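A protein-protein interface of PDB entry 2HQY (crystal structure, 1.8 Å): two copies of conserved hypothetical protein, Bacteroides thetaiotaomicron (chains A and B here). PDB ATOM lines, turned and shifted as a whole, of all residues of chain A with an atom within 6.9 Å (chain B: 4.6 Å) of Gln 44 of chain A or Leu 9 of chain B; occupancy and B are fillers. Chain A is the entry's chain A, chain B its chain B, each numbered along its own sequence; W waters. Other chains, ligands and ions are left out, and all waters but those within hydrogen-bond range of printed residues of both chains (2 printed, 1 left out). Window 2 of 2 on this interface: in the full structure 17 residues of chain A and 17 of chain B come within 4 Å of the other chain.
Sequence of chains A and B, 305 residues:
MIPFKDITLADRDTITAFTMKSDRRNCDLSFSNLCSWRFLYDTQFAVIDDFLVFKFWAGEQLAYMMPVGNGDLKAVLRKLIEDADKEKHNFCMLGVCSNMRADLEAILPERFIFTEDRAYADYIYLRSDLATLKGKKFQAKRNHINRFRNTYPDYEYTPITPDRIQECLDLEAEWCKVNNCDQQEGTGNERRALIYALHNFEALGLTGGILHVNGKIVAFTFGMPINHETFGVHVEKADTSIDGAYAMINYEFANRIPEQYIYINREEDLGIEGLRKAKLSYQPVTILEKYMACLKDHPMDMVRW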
ATOM      1  N   PHE A   4      21.583 -21.748 -11.408  1.00  0.00           N
ATOM      2  CA  PHE A   4      22.916 -21.895 -12.006  1.00  0.00           C
ATOM      3  C   PHE A   4      22.775 -22.302 -13.461  1.00  0.00           C
ATOM      4  O   PHE A   4      21.943 -23.163 -13.812  1.00  0.00           O
ATOM      5  CB  PHE A   4      23.781 -22.913 -11.253  1.00  0.00           C
ATOM      6  CG  PHE A   4      24.455 -22.358 -10.040  1.00  0.00           C
ATOM      7  CD1 PHE A   4      25.475 -21.416 -10.169  1.00  0.00           C
ATOM      8  CD2 PHE A   4      24.049 -22.743  -8.756  1.00  0.00           C
ATOM      9  CE1 PHE A   4      26.095 -20.870  -9.042  1.00  0.00           C
ATOM     10  CE2 PHE A   4      24.672 -22.216  -7.618  1.00  0.00           C
ATOM     11  CZ  PHE A   4      25.694 -21.282  -7.753  1.00  0.00           C
ATOM     12  N   LYS A   5      23.614 -21.705 -14.299  1.00  0.00           N
ATOM     13  CA  LYS A   5      23.669 -22.094 -15.688  1.00  0.00           C
ATOM     14  C   LYS A   5      25.091 -22.315 -16.144  1.00  0.00           C
ATOM     15  O   LYS A   5      26.018 -21.672 -15.647  1.00  0.00           O
ATOM     16  CB  LYS A   5      22.983 -21.065 -16.574  1.00  0.00           C
ATOM     17  CG  LYS A   5      23.263 -19.633 -16.271  1.00  0.00           C
ATOM     18  CD  LYS A   5      21.957 -18.842 -16.417  1.00  0.00           C
ATOM     19  N   ASP A   6      25.245 -23.221 -17.100  1.00  0.00           N
ATOM     20  CA  ASP A   6      26.561 -23.475 -17.691  1.00  0.00           C
ATOM     21  C   ASP A   6      27.112 -22.201 -18.312  1.00  0.00           C
ATOM     22  O   ASP A   6      26.422 -21.493 -19.045  1.00  0.00           O
ATOM     23  CB  ASP A   6      26.477 -24.555 -18.770  1.00  0.00           C
ATOM     24  CG  ASP A   6      25.919 -25.848 -18.261  1.00  0.00           C
ATOM     25  OD1 ASP A   6      25.925 -26.092 -17.027  1.00  0.00           O
ATOM     26  OD2 ASP A   6      25.441 -26.623 -19.119  1.00  0.00           O
ATOM     27  N   ILE A   7      28.387 -21.920 -18.064  1.00  0.00           N
ATOM     28  CA  ILE A   7      29.002 -20.761 -18.685  1.00  0.00           C
ATOM     29  C   ILE A   7      29.183 -21.004 -20.200  1.00  0.00           C
ATOM     30  O   ILE A   7      29.493 -22.116 -20.624  1.00  0.00           O
ATOM     31  CB  ILE A   7      30.346 -20.412 -18.014  1.00  0.00           C
ATOM     32  CG1 ILE A   7      30.752 -18.980 -18.438  1.00  0.00           C
ATOM     33  CG2 ILE A   7      31.396 -21.524 -18.295  1.00  0.00           C
ATOM     34  CD1 ILE A   7      31.994 -18.395 -17.789  1.00  0.00           C
ATOM     35  N   LEU A  34      37.530 -18.920 -17.739  1.00  0.00           N
ATOM     36  CA  LEU A  34      36.276 -19.507 -17.263  1.00  0.00           C
ATOM     37  C   LEU A  34      35.658 -20.435 -18.321  1.00  0.00           C
ATOM     38  O   LEU A  34      35.257 -21.556 -17.996  1.00  0.00           O
ATOM     39  CB  LEU A  34      35.277 -18.407 -16.870  1.00  0.00           C
ATOM     40  CG  LEU A  34      35.649 -17.689 -15.564  1.00  0.00           C
ATOM     41  CD1 LEU A  34      34.941 -16.339 -15.488  1.00  0.00           C
ATOM     42  CD2 LEU A  34      35.308 -18.531 -14.332  1.00  0.00           C
ATOM     43  N   ARG A  38      35.988 -24.915 -18.672  1.00  0.00           N
ATOM     44  CA  ARG A  38      34.687 -25.509 -18.343  1.00  0.00           C
ATOM     45  C   ARG A  38      34.684 -27.044 -18.567  1.00  0.00           C
ATOM     46  O   ARG A  38      33.983 -27.789 -17.874  1.00  0.00           O
ATOM     47  CB  ARG A  38      33.598 -24.847 -19.189  1.00  0.00           C
ATOM     48  CG  ARG A  38      32.140 -25.284 -18.846  1.00  0.00           C
ATOM     49  CD  ARG A  38      31.176 -24.798 -19.938  1.00  0.00           C
ATOM     50  NE  ARG A  38      31.562 -25.390 -21.217  1.00  0.00           N
ATOM     51  CZ  ARG A  38      31.355 -24.853 -22.410  1.00  0.00           C
ATOM     52  NH1 ARG A  38      30.702 -23.695 -22.530  1.00  0.00           N
ATOM     53  NH2 ARG A  38      31.787 -25.518 -23.494  1.00  0.00           N
ATOM     54  N   TYR A  41      35.770 -28.608 -15.259  1.00  0.00           N
ATOM     55  CA  TYR A  41      35.046 -28.306 -13.995  1.00  0.00           C
ATOM     56  C   TYR A  41      33.527 -28.248 -14.086  1.00  0.00           C
ATOM     57  O   TYR A  41      32.859 -27.950 -13.093  1.00  0.00           O
ATOM     58  CB  TYR A  41      35.543 -26.966 -13.448  1.00  0.00           C
ATOM     59  CG  TYR A  41      37.033 -26.960 -13.208  1.00  0.00           C
ATOM     60  CD1 TYR A  41      37.615 -27.884 -12.327  1.00  0.00           C
ATOM     61  CD2 TYR A  41      37.859 -26.035 -13.851  1.00  0.00           C
ATOM     62  CE1 TYR A  41      39.011 -27.880 -12.104  1.00  0.00           C
ATOM     63  CE2 TYR A  41      39.250 -26.026 -13.636  1.00  0.00           C
ATOM     64  CZ  TYR A  41      39.808 -26.953 -12.766  1.00  0.00           C
ATOM     65  OH  TYR A  41      41.178 -26.955 -12.540  1.00  0.00           O
ATOM     66  N   ASP A  42      32.982 -28.479 -15.279  1.00  0.00           N
ATOM     67  CA  ASP A  42      31.524 -28.378 -15.491  1.00  0.00           C
ATOM     68  C   ASP A  42      30.997 -27.043 -14.941  1.00  0.00           C
ATOM     69  O   ASP A  42      29.964 -26.991 -14.277  1.00  0.00           O
ATOM     70  CB  ASP A  42      30.792 -29.554 -14.828  1.00  0.00           C
ATOM     71  CG  ASP A  42      31.011 -30.882 -15.552  1.00  0.00           C
ATOM     72  OD1 ASP A  42      31.597 -30.929 -16.667  1.00  0.00           O
ATOM     73  OD2 ASP A  42      30.572 -31.891 -14.974  1.00  0.00           O
ATOM     74  N   THR A  43      31.721 -25.970 -15.235  1.00  0.00           N
ATOM     75  CA  THR A  43      31.549 -24.643 -14.628  1.00  0.00           C
ATOM     76  C   THR A  43      30.170 -24.027 -14.880  1.00  0.00           C
ATOM     77  O   THR A  43      29.691 -24.009 -16.023  1.00  0.00           O
ATOM     78  CB  THR A  43      32.682 -23.736 -15.131  1.00  0.00           C
ATOM     79  OG1 THR A  43      33.927 -24.401 -14.822  1.00  0.00           O
ATOM     80  CG2 THR A  43      32.636 -22.344 -14.515  1.00  0.00           C
ATOM     81  N   GLN A  44      29.555 -23.542 -13.807  1.00  0.00           N
ATOM     82  CA  GLN A  44      28.272 -22.824 -13.913  1.00  0.00           C
ATOM     83  C   GLN A  44      28.373 -21.462 -13.225  1.00  0.00           C
ATOM     84  O   GLN A  44      29.285 -21.234 -12.422  1.00  0.00           O
ATOM     85  CB  GLN A  44      27.144 -23.690 -13.328  1.00  0.00           C
ATOM     86  CG  GLN A  44      26.979 -24.993 -14.052  1.00  0.00           C
ATOM     87  CD  GLN A  44      25.877 -25.884 -13.456  1.00  0.00           C
ATOM     88  OE1 GLN A  44      25.601 -25.857 -12.260  1.00  0.00           O
ATOM     89  NE2 GLN A  44      25.267 -26.715 -14.318  1.00  0.00           N
ATOM     90  N   PHE A  45      27.455 -20.557 -13.543  1.00  0.00           N
ATOM     91  CA  PHE A  45      27.388 -19.266 -12.864  1.00  0.00           C
ATOM     92  C   PHE A  45      25.938 -18.861 -12.638  1.00  0.00           C
ATOM     93  O   PHE A  45      25.005 -19.388 -13.258  1.00  0.00           O
ATOM     94  CB  PHE A  45      28.109 -18.155 -13.645  1.00  0.00           C
ATOM     95  CG  PHE A  45      27.336 -17.648 -14.836  1.00  0.00           C
ATOM     96  CD1 PHE A  45      26.597 -16.463 -14.761  1.00  0.00           C
ATOM     97  CD2 PHE A  45      27.316 -18.379 -16.015  1.00  0.00           C
ATOM     98  CE1 PHE A  45      25.871 -16.010 -15.852  1.00  0.00           C
ATOM     99  CE2 PHE A  45      26.589 -17.932 -17.124  1.00  0.00           C
ATOM    100  CZ  PHE A  45      25.867 -16.743 -17.047  1.00  0.00           C
ATOM    101  N   ALA A  46      25.780 -17.890 -11.757  1.00  0.00           N
ATOM    102  CA  ALA A  46      24.500 -17.245 -11.539  1.00  0.00           C
ATOM    103  C   ALA A  46      24.752 -15.835 -11.055  1.00  0.00           C
ATOM    104  O   ALA A  46      25.788 -15.545 -10.463  1.00  0.00           O
ATOM    105  CB  ALA A  46      23.667 -18.025 -10.535  1.00  0.00           C
ATOM    106  N   VAL A  53      28.244 -15.245  -9.064  1.00  0.00           N
ATOM    107  CA  VAL A  53      28.778 -16.431  -8.361  1.00  0.00           C
ATOM    108  C   VAL A  53      29.057 -17.602  -9.308  1.00  0.00           C
ATOM    109  O   VAL A  53      28.336 -17.780 -10.270  1.00  0.00           O
ATOM    110  CB  VAL A  53      27.810 -16.839  -7.217  1.00  0.00           C
ATOM    111  CG1 VAL A  53      27.759 -15.725  -6.146  1.00  0.00           C
ATOM    112  CG2 VAL A  53      26.392 -17.069  -7.758  1.00  0.00           C
ATOM    113  N   PHE A  54      30.118 -18.370  -9.052  1.00  0.00           N
ATOM    114  CA  PHE A  54      30.515 -19.492  -9.927  1.00  0.00           C
ATOM    115  C   PHE A  54      30.507 -20.759  -9.081  1.00  0.00           C
ATOM    116  O   PHE A  54      30.748 -20.697  -7.865  1.00  0.00           O
ATOM    117  CB  PHE A  54      31.895 -19.280 -10.537  1.00  0.00           C
ATOM    118  CG  PHE A  54      31.967 -18.136 -11.515  1.00  0.00           C
ATOM    119  CD1 PHE A  54      31.576 -18.313 -12.842  1.00  0.00           C
ATOM    120  CD2 PHE A  54      32.392 -16.875 -11.100  1.00  0.00           C
ATOM    121  CE1 PHE A  54      31.633 -17.241 -13.777  1.00  0.00           C
ATOM    122  CE2 PHE A  54      32.453 -15.788 -12.021  1.00  0.00           C
ATOM    123  CZ  PHE A  54      32.068 -15.975 -13.358  1.00  0.00           C
ATOM    124  N   LYS A  55      30.186 -21.882  -9.732  1.00  0.00           N
ATOM    125  CA  LYS A  55      30.113 -23.214  -9.100  1.00  0.00           C
ATOM    126  C   LYS A  55      30.892 -24.159 -10.019  1.00  0.00           C
ATOM    127  O   LYS A  55      30.664 -24.144 -11.256  1.00  0.00           O
ATOM    128  CB  LYS A  55      28.651 -23.622  -8.962  1.00  0.00           C
ATOM    129  CG  LYS A  55      28.350 -25.034  -8.458  1.00  0.00           C
ATOM    130  CD  LYS A  55      26.834 -25.180  -8.359  1.00  0.00           C
ATOM    131  CE  LYS A  55      26.380 -26.507  -7.709  1.00  0.00           C
ATOM    132  NZ  LYS A  55      24.862 -26.559  -7.647  1.00  0.00           N
ATOM    133  N   PHE A  56      31.823 -24.910  -9.417  1.00  0.00           N
ATOM    134  CA  PHE A  56      32.789 -25.806 -10.102  1.00  0.00           C
ATOM    135  C   PHE A  56      32.788 -27.173  -9.439  1.00  0.00           C
ATOM    136  O   PHE A  56      32.660 -27.275  -8.212  1.00  0.00           O
ATOM    137  CB  PHE A  56      34.274 -25.369  -9.926  1.00  0.00           C
ATOM    138  CG  PHE A  56      34.555 -23.971 -10.294  1.00  0.00           C
ATOM    139  CD1 PHE A  56      34.949 -23.645 -11.614  1.00  0.00           C
ATOM    140  CD2 PHE A  56      34.498 -22.975  -9.333  1.00  0.00           C
ATOM    141  CE1 PHE A  56      35.233 -22.302 -11.977  1.00  0.00           C
ATOM    142  CE2 PHE A  56      34.781 -21.638  -9.678  1.00  0.00           C
ATOM    143  CZ  PHE A  56      35.136 -21.292 -10.986  1.00  0.00           C
ATOM    144  N   TRP A  57      33.024 -28.206 -10.234  1.00  0.00           N
ATOM    145  CA  TRP A  57      33.309 -29.526  -9.699  1.00  0.00           C
ATOM    146  C   TRP A  57      34.758 -29.840 -10.058  1.00  0.00           C
ATOM    147  O   TRP A  57      35.084 -30.034 -11.233  1.00  0.00           O
ATOM    148  CB  TRP A  57      32.373 -30.572 -10.305  1.00  0.00           C
ATOM    149  CG  TRP A  57      30.952 -30.404  -9.828  1.00  0.00           C
ATOM    150  CD1 TRP A  57      29.967 -29.670 -10.435  1.00  0.00           C
ATOM    151  CD2 TRP A  57      30.369 -30.962  -8.641  1.00  0.00           C
ATOM    152  NE1 TRP A  57      28.794 -29.759  -9.708  1.00  0.00           N
ATOM    153  CE2 TRP A  57      29.017 -30.525  -8.594  1.00  0.00           C
ATOM    154  CE3 TRP A  57      30.858 -31.776  -7.605  1.00  0.00           C
ATOM    155  CZ2 TRP A  57      28.143 -30.903  -7.566  1.00  0.00           C
ATOM    156  CZ3 TRP A  57      29.982 -32.153  -6.576  1.00  0.00           C
ATOM    157  CH2 TRP A  57      28.637 -31.708  -6.572  1.00  0.00           C
ATOM    158  N   GLU A  87      23.588 -30.209  -2.570  1.00  0.00           N
ATOM    159  CA  GLU A  87      24.533 -31.065  -3.255  1.00  0.00           C
ATOM    160  C   GLU A  87      25.116 -32.139  -2.337  1.00  0.00           C
ATOM    161  O   GLU A  87      25.804 -33.046  -2.820  1.00  0.00           O
ATOM    162  CB  GLU A  87      25.657 -30.223  -3.875  1.00  0.00           C
ATOM    163  CG  GLU A  87      25.160 -29.231  -4.926  1.00  0.00           C
ATOM    164  CD  GLU A  87      24.689 -29.894  -6.223  1.00  0.00           C
ATOM    165  OE1 GLU A  87      24.703 -31.148  -6.339  1.00  0.00           O
ATOM    166  OE2 GLU A  87      24.308 -29.147  -7.140  1.00  0.00           O
ATOM    167  N   THR B   8      24.109 -25.634 -23.693  1.00  0.00           N
ATOM    168  CA  THR B   8      23.967 -25.562 -22.234  1.00  0.00           C
ATOM    169  C   THR B   8      22.620 -26.103 -21.792  1.00  0.00           C
ATOM    170  O   THR B   8      21.707 -26.278 -22.610  1.00  0.00           O
ATOM    171  CB  THR B   8      24.008 -24.122 -21.700  1.00  0.00           C
ATOM    172  OG1 THR B   8      22.752 -23.475 -21.952  1.00  0.00           O
ATOM    173  CG2 THR B   8      25.138 -23.334 -22.313  1.00  0.00           C
ATOM    174  N   LEU B   9      22.491 -26.356 -20.480  1.00  0.00           N
ATOM    175  CA  LEU B   9      21.181 -26.742 -19.910  1.00  0.00           C
ATOM    176  C   LEU B   9      20.024 -25.849 -20.357  1.00  0.00           C
ATOM    177  O   LEU B   9      18.896 -26.322 -20.565  1.00  0.00           O
ATOM    178  CB  LEU B   9      21.257 -26.680 -18.388  1.00  0.00           C
ATOM    179  CG  LEU B   9      22.287 -27.591 -17.771  1.00  0.00           C
ATOM    180  CD1 LEU B   9      22.384 -27.356 -16.249  1.00  0.00           C
ATOM    181  CD2 LEU B   9      21.904 -29.028 -18.106  1.00  0.00           C
ATOM    182  N   ALA B  10      20.285 -24.550 -20.479  1.00  0.00           N
ATOM    183  CA  ALA B  10      19.221 -23.604 -20.813  1.00  0.00           C
ATOM    184  C   ALA B  10      18.701 -23.746 -22.259  1.00  0.00           C
ATOM    185  O   ALA B  10      17.690 -23.145 -22.624  1.00  0.00           O
ATOM    186  CB  ALA B  10      19.698 -22.175 -20.549  1.00  0.00           C
ATOM    187  N   ASP B  11      19.392 -24.541 -23.076  1.00  0.00           N
ATOM    188  CA  ASP B  11      18.999 -24.749 -24.477  1.00  0.00           C
ATOM    189  C   ASP B  11      18.056 -25.934 -24.690  1.00  0.00           C
ATOM    190  O   ASP B  11      17.758 -26.293 -25.831  1.00  0.00           O
ATOM    191  CB  ASP B  11      20.244 -24.888 -25.354  1.00  0.00           C
ATOM    192  CG  ASP B  11      21.126 -23.668 -25.282  1.00  0.00           C
ATOM    193  OD1 ASP B  11      20.616 -22.525 -25.518  1.00  0.00           O
ATOM    194  OD2 ASP B  11      22.330 -23.856 -24.991  1.00  0.00           O
ATOM    195  N   ARG B  12      17.559 -26.499 -23.595  1.00  0.00           N
ATOM    196  CA  ARG B  12      16.710 -27.669 -23.656  1.00  0.00           C
ATOM    197  C   ARG B  12      15.480 -27.443 -24.566  1.00  0.00           C
ATOM    198  O   ARG B  12      15.228 -28.242 -25.456  1.00  0.00           O
ATOM    199  CB  ARG B  12      16.266 -28.083 -22.258  1.00  0.00           C
ATOM    200  CG  ARG B  12      15.401 -29.309 -22.274  1.00  0.00           C
ATOM    201  CD  ARG B  12      15.053 -29.602 -20.813  1.00  0.00           C
ATOM    202  NE  ARG B  12      13.831 -30.349 -20.641  1.00  0.00           N
ATOM    203  CZ  ARG B  12      13.349 -30.696 -19.446  1.00  0.00           C
ATOM    204  NH1 ARG B  12      13.999 -30.328 -18.337  1.00  0.00           N
ATOM    205  NH2 ARG B  12      12.224 -31.407 -19.360  1.00  0.00           N
ATOM    206  N   PHE B  31      18.950 -34.768 -25.623  1.00  0.00           N
ATOM    207  CA  PHE B  31      19.483 -33.542 -24.987  1.00  0.00           C
ATOM    208  C   PHE B  31      20.494 -33.870 -23.886  1.00  0.00           C
ATOM    209  O   PHE B  31      21.536 -33.213 -23.801  1.00  0.00           O
ATOM    210  CB  PHE B  31      18.370 -32.685 -24.394  1.00  0.00           C
ATOM    211  CG  PHE B  31      18.863 -31.386 -23.845  1.00  0.00           C
ATOM    212  CD1 PHE B  31      19.471 -30.422 -24.679  1.00  0.00           C
ATOM    213  CD2 PHE B  31      18.733 -31.111 -22.495  1.00  0.00           C
ATOM    214  CE1 PHE B  31      19.937 -29.188 -24.107  1.00  0.00           C
ATOM    215  CE2 PHE B  31      19.199 -29.880 -21.951  1.00  0.00           C
ATOM    216  CZ  PHE B  31      19.788 -28.953 -22.751  1.00  0.00           C
ATOM    217  N   CYS B  35      24.464 -32.633 -23.915  1.00  0.00           N
ATOM    218  CA  CYS B  35      25.069 -31.814 -22.831  1.00  0.00           C
ATOM    219  C   CYS B  35      26.139 -32.572 -22.074  1.00  0.00           C
ATOM    220  O   CYS B  35      27.150 -31.976 -21.714  1.00  0.00           O
ATOM    221  CB  CYS B  35      24.039 -31.291 -21.802  1.00  0.00           C
ATOM    222  SG  CYS B  35      22.915 -30.097 -22.481  1.00  0.00           S
ATOM    223  N   TYR B 196      28.066 -35.491 -14.936  1.00  0.00           N
ATOM    224  CA  TYR B 196      27.325 -34.309 -15.414  1.00  0.00           C
ATOM    225  C   TYR B 196      25.829 -34.623 -15.401  1.00  0.00           C
ATOM    226  O   TYR B 196      25.015 -33.827 -14.921  1.00  0.00           O
ATOM    227  CB  TYR B 196      27.772 -33.918 -16.823  1.00  0.00           C
ATOM    228  CG  TYR B 196      27.067 -32.696 -17.343  1.00  0.00           C
ATOM    229  CD1 TYR B 196      27.627 -31.423 -17.170  1.00  0.00           C
ATOM    230  CD2 TYR B 196      25.827 -32.803 -17.997  1.00  0.00           C
ATOM    231  CE1 TYR B 196      26.979 -30.289 -17.641  1.00  0.00           C
ATOM    232  CE2 TYR B 196      25.173 -31.680 -18.464  1.00  0.00           C
ATOM    233  CZ  TYR B 196      25.743 -30.428 -18.281  1.00  0.00           C
ATOM    234  OH  TYR B 196      25.108 -29.313 -18.779  1.00  0.00           O
ATOM    235  N   ASN B 200      23.017 -32.819 -12.989  1.00  0.00           N
ATOM    236  CA  ASN B 200      22.060 -31.895 -13.613  1.00  0.00           C
ATOM    237  C   ASN B 200      20.778 -32.609 -14.028  1.00  0.00           C
ATOM    238  O   ASN B 200      20.123 -32.228 -14.992  1.00  0.00           O
ATOM    239  CB  ASN B 200      22.739 -31.196 -14.803  1.00  0.00           C
ATOM    240  CG  ASN B 200      23.910 -30.339 -14.345  1.00  0.00           C
ATOM    241  OD1 ASN B 200      23.712 -29.305 -13.713  1.00  0.00           O
ATOM    242  ND2 ASN B 200      25.140 -30.794 -14.625  1.00  0.00           N
ATOM    243  N   ALA B 203      17.318 -30.612 -14.565  1.00  0.00           N
ATOM    244  CA  ALA B 203      17.490 -29.600 -15.621  1.00  0.00           C
ATOM    245  C   ALA B 203      17.517 -30.241 -17.017  1.00  0.00           C
ATOM    246  O   ALA B 203      16.996 -29.675 -17.999  1.00  0.00           O
ATOM    247  CB  ALA B 203      18.783 -28.778 -15.370  1.00  0.00           C
ATOM    248  N   LEU B 204      18.134 -31.417 -17.094  1.00  0.00           N
ATOM    249  CA  LEU B 204      18.266 -32.127 -18.365  1.00  0.00           C
ATOM    250  C   LEU B 204      16.953 -32.735 -18.829  1.00  0.00           C
ATOM    251  O   LEU B 204      16.763 -32.892 -20.032  1.00  0.00           O
ATOM    252  CB  LEU B 204      19.322 -33.232 -18.294  1.00  0.00           C
ATOM    253  CG  LEU B 204      20.766 -32.704 -18.201  1.00  0.00           C
ATOM    254  CD1 LEU B 204      21.696 -33.803 -17.818  1.00  0.00           C
ATOM    255  CD2 LEU B 204      21.147 -32.081 -19.553  1.00  0.00           C
HETATM  256  O   HOH W   1      22.445 -23.317 -18.710  1.00  0.00           O
HETATM  257  O   HOH W   2      27.504 -29.241 -13.427  1.00  0.00           O
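Printed residues of chain B within 4 Å of Asp 6 of chain A: Thr 8, Leu 9 and Tyr 196. Of the printed residues of chain B, Asp 42 of chain A touches Tyr 196. Of the printed residues of chain B, Gln 44 of chain A touches Leu 9 and Asn 200. Leu 9 of chain B touches just these residues of chain A: Asp 6 (3.3 Å) and Gln 44 (3.5 Å). The nearest printed residue of chain B that does not touch Gln 44 of chain A is Tyr 196 of chain B (5.2 Å). The nearest printed residue of chain A that does not touch Thr 8 of chain B is Ile 7 of chain A (4.8 Å).
The side-chain carboxylate (OD1) of Asp 6 of chain A lies within hydrogen-bond range of the side-chain amide nitrogen (NE2) of Gln 44 of chain A (2.9 Å). The backbone carbonyl oxygen of Lys 55 of chain A sits at hydrogen-bond distance from the backbone NH of Gln 44 of chain A, at 2.8 Å. N of Ala 10 of chain B lies within hydrogen-bond range of OG1 of Thr 8 of chain B, at 3.1 Å. N of Thr 8 of chain B sits at hydrogen-bond distance from OD2 of Asp 11 of chain B (2.8 Å). The backbone carbonyl oxygen (O) of Tyr 196 of chain B is in hydrogen-bond range of the side-chain amide nitrogen (ND2) of Asn 200 of chain B.
Thr 8 of chain B touches Asp 6 of chain A (CA to OD2, 3.6 Å). CD1 of Tyr 196 of chain B touches OD2 of Asp 42 of chain A, 3.7 Å away. Gln 44 of chain A touches Leu 9 of chain B (NE2 to CD1, 3.5 Å).
OD2 of Asp 6 of chain A is in hydrogen-bond range of N of Leu 9 of chain B, at 3.3 Å. The side-chain carboxylate of Asp 6 of chain A sits at hydrogen-bond distance from the side-chain hydroxyl of Tyr 196 of chain B (2.7 Å). The side-chain amide nitrogen of Gln 44 of chain A is in hydrogen-bond range of the side-chain amide oxygen of Asn 200 of chain B, 3.1 Å away.
Printed residues of chain A that touch a printed residue of chain B: Asp 6, Asp 42 and Gln 44. Of the 11 printed residues of chain B, 4 touch a printed residue of chain A. Among the printed residues, 6 pairs touch across the chains.
Water W1 lies within hydrogen-bond range of the backbone NH (N) of Ala 10 of chain B (3.1 Å), the backbone NH (N) of Asp 6 of chain A (3.2 Å) and the side-chain hydroxyl (OG1) of Thr 8 of chain B (3.3 Å). Water W2 lies within hydrogen-bond range of ND2 of Asn 200 of chain B (3.1 Å), O of Asp 42 of chain A (3.4 Å) and NE2 of Gln 44 of chain A (3.5 Å).
No position is printed for both chains.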
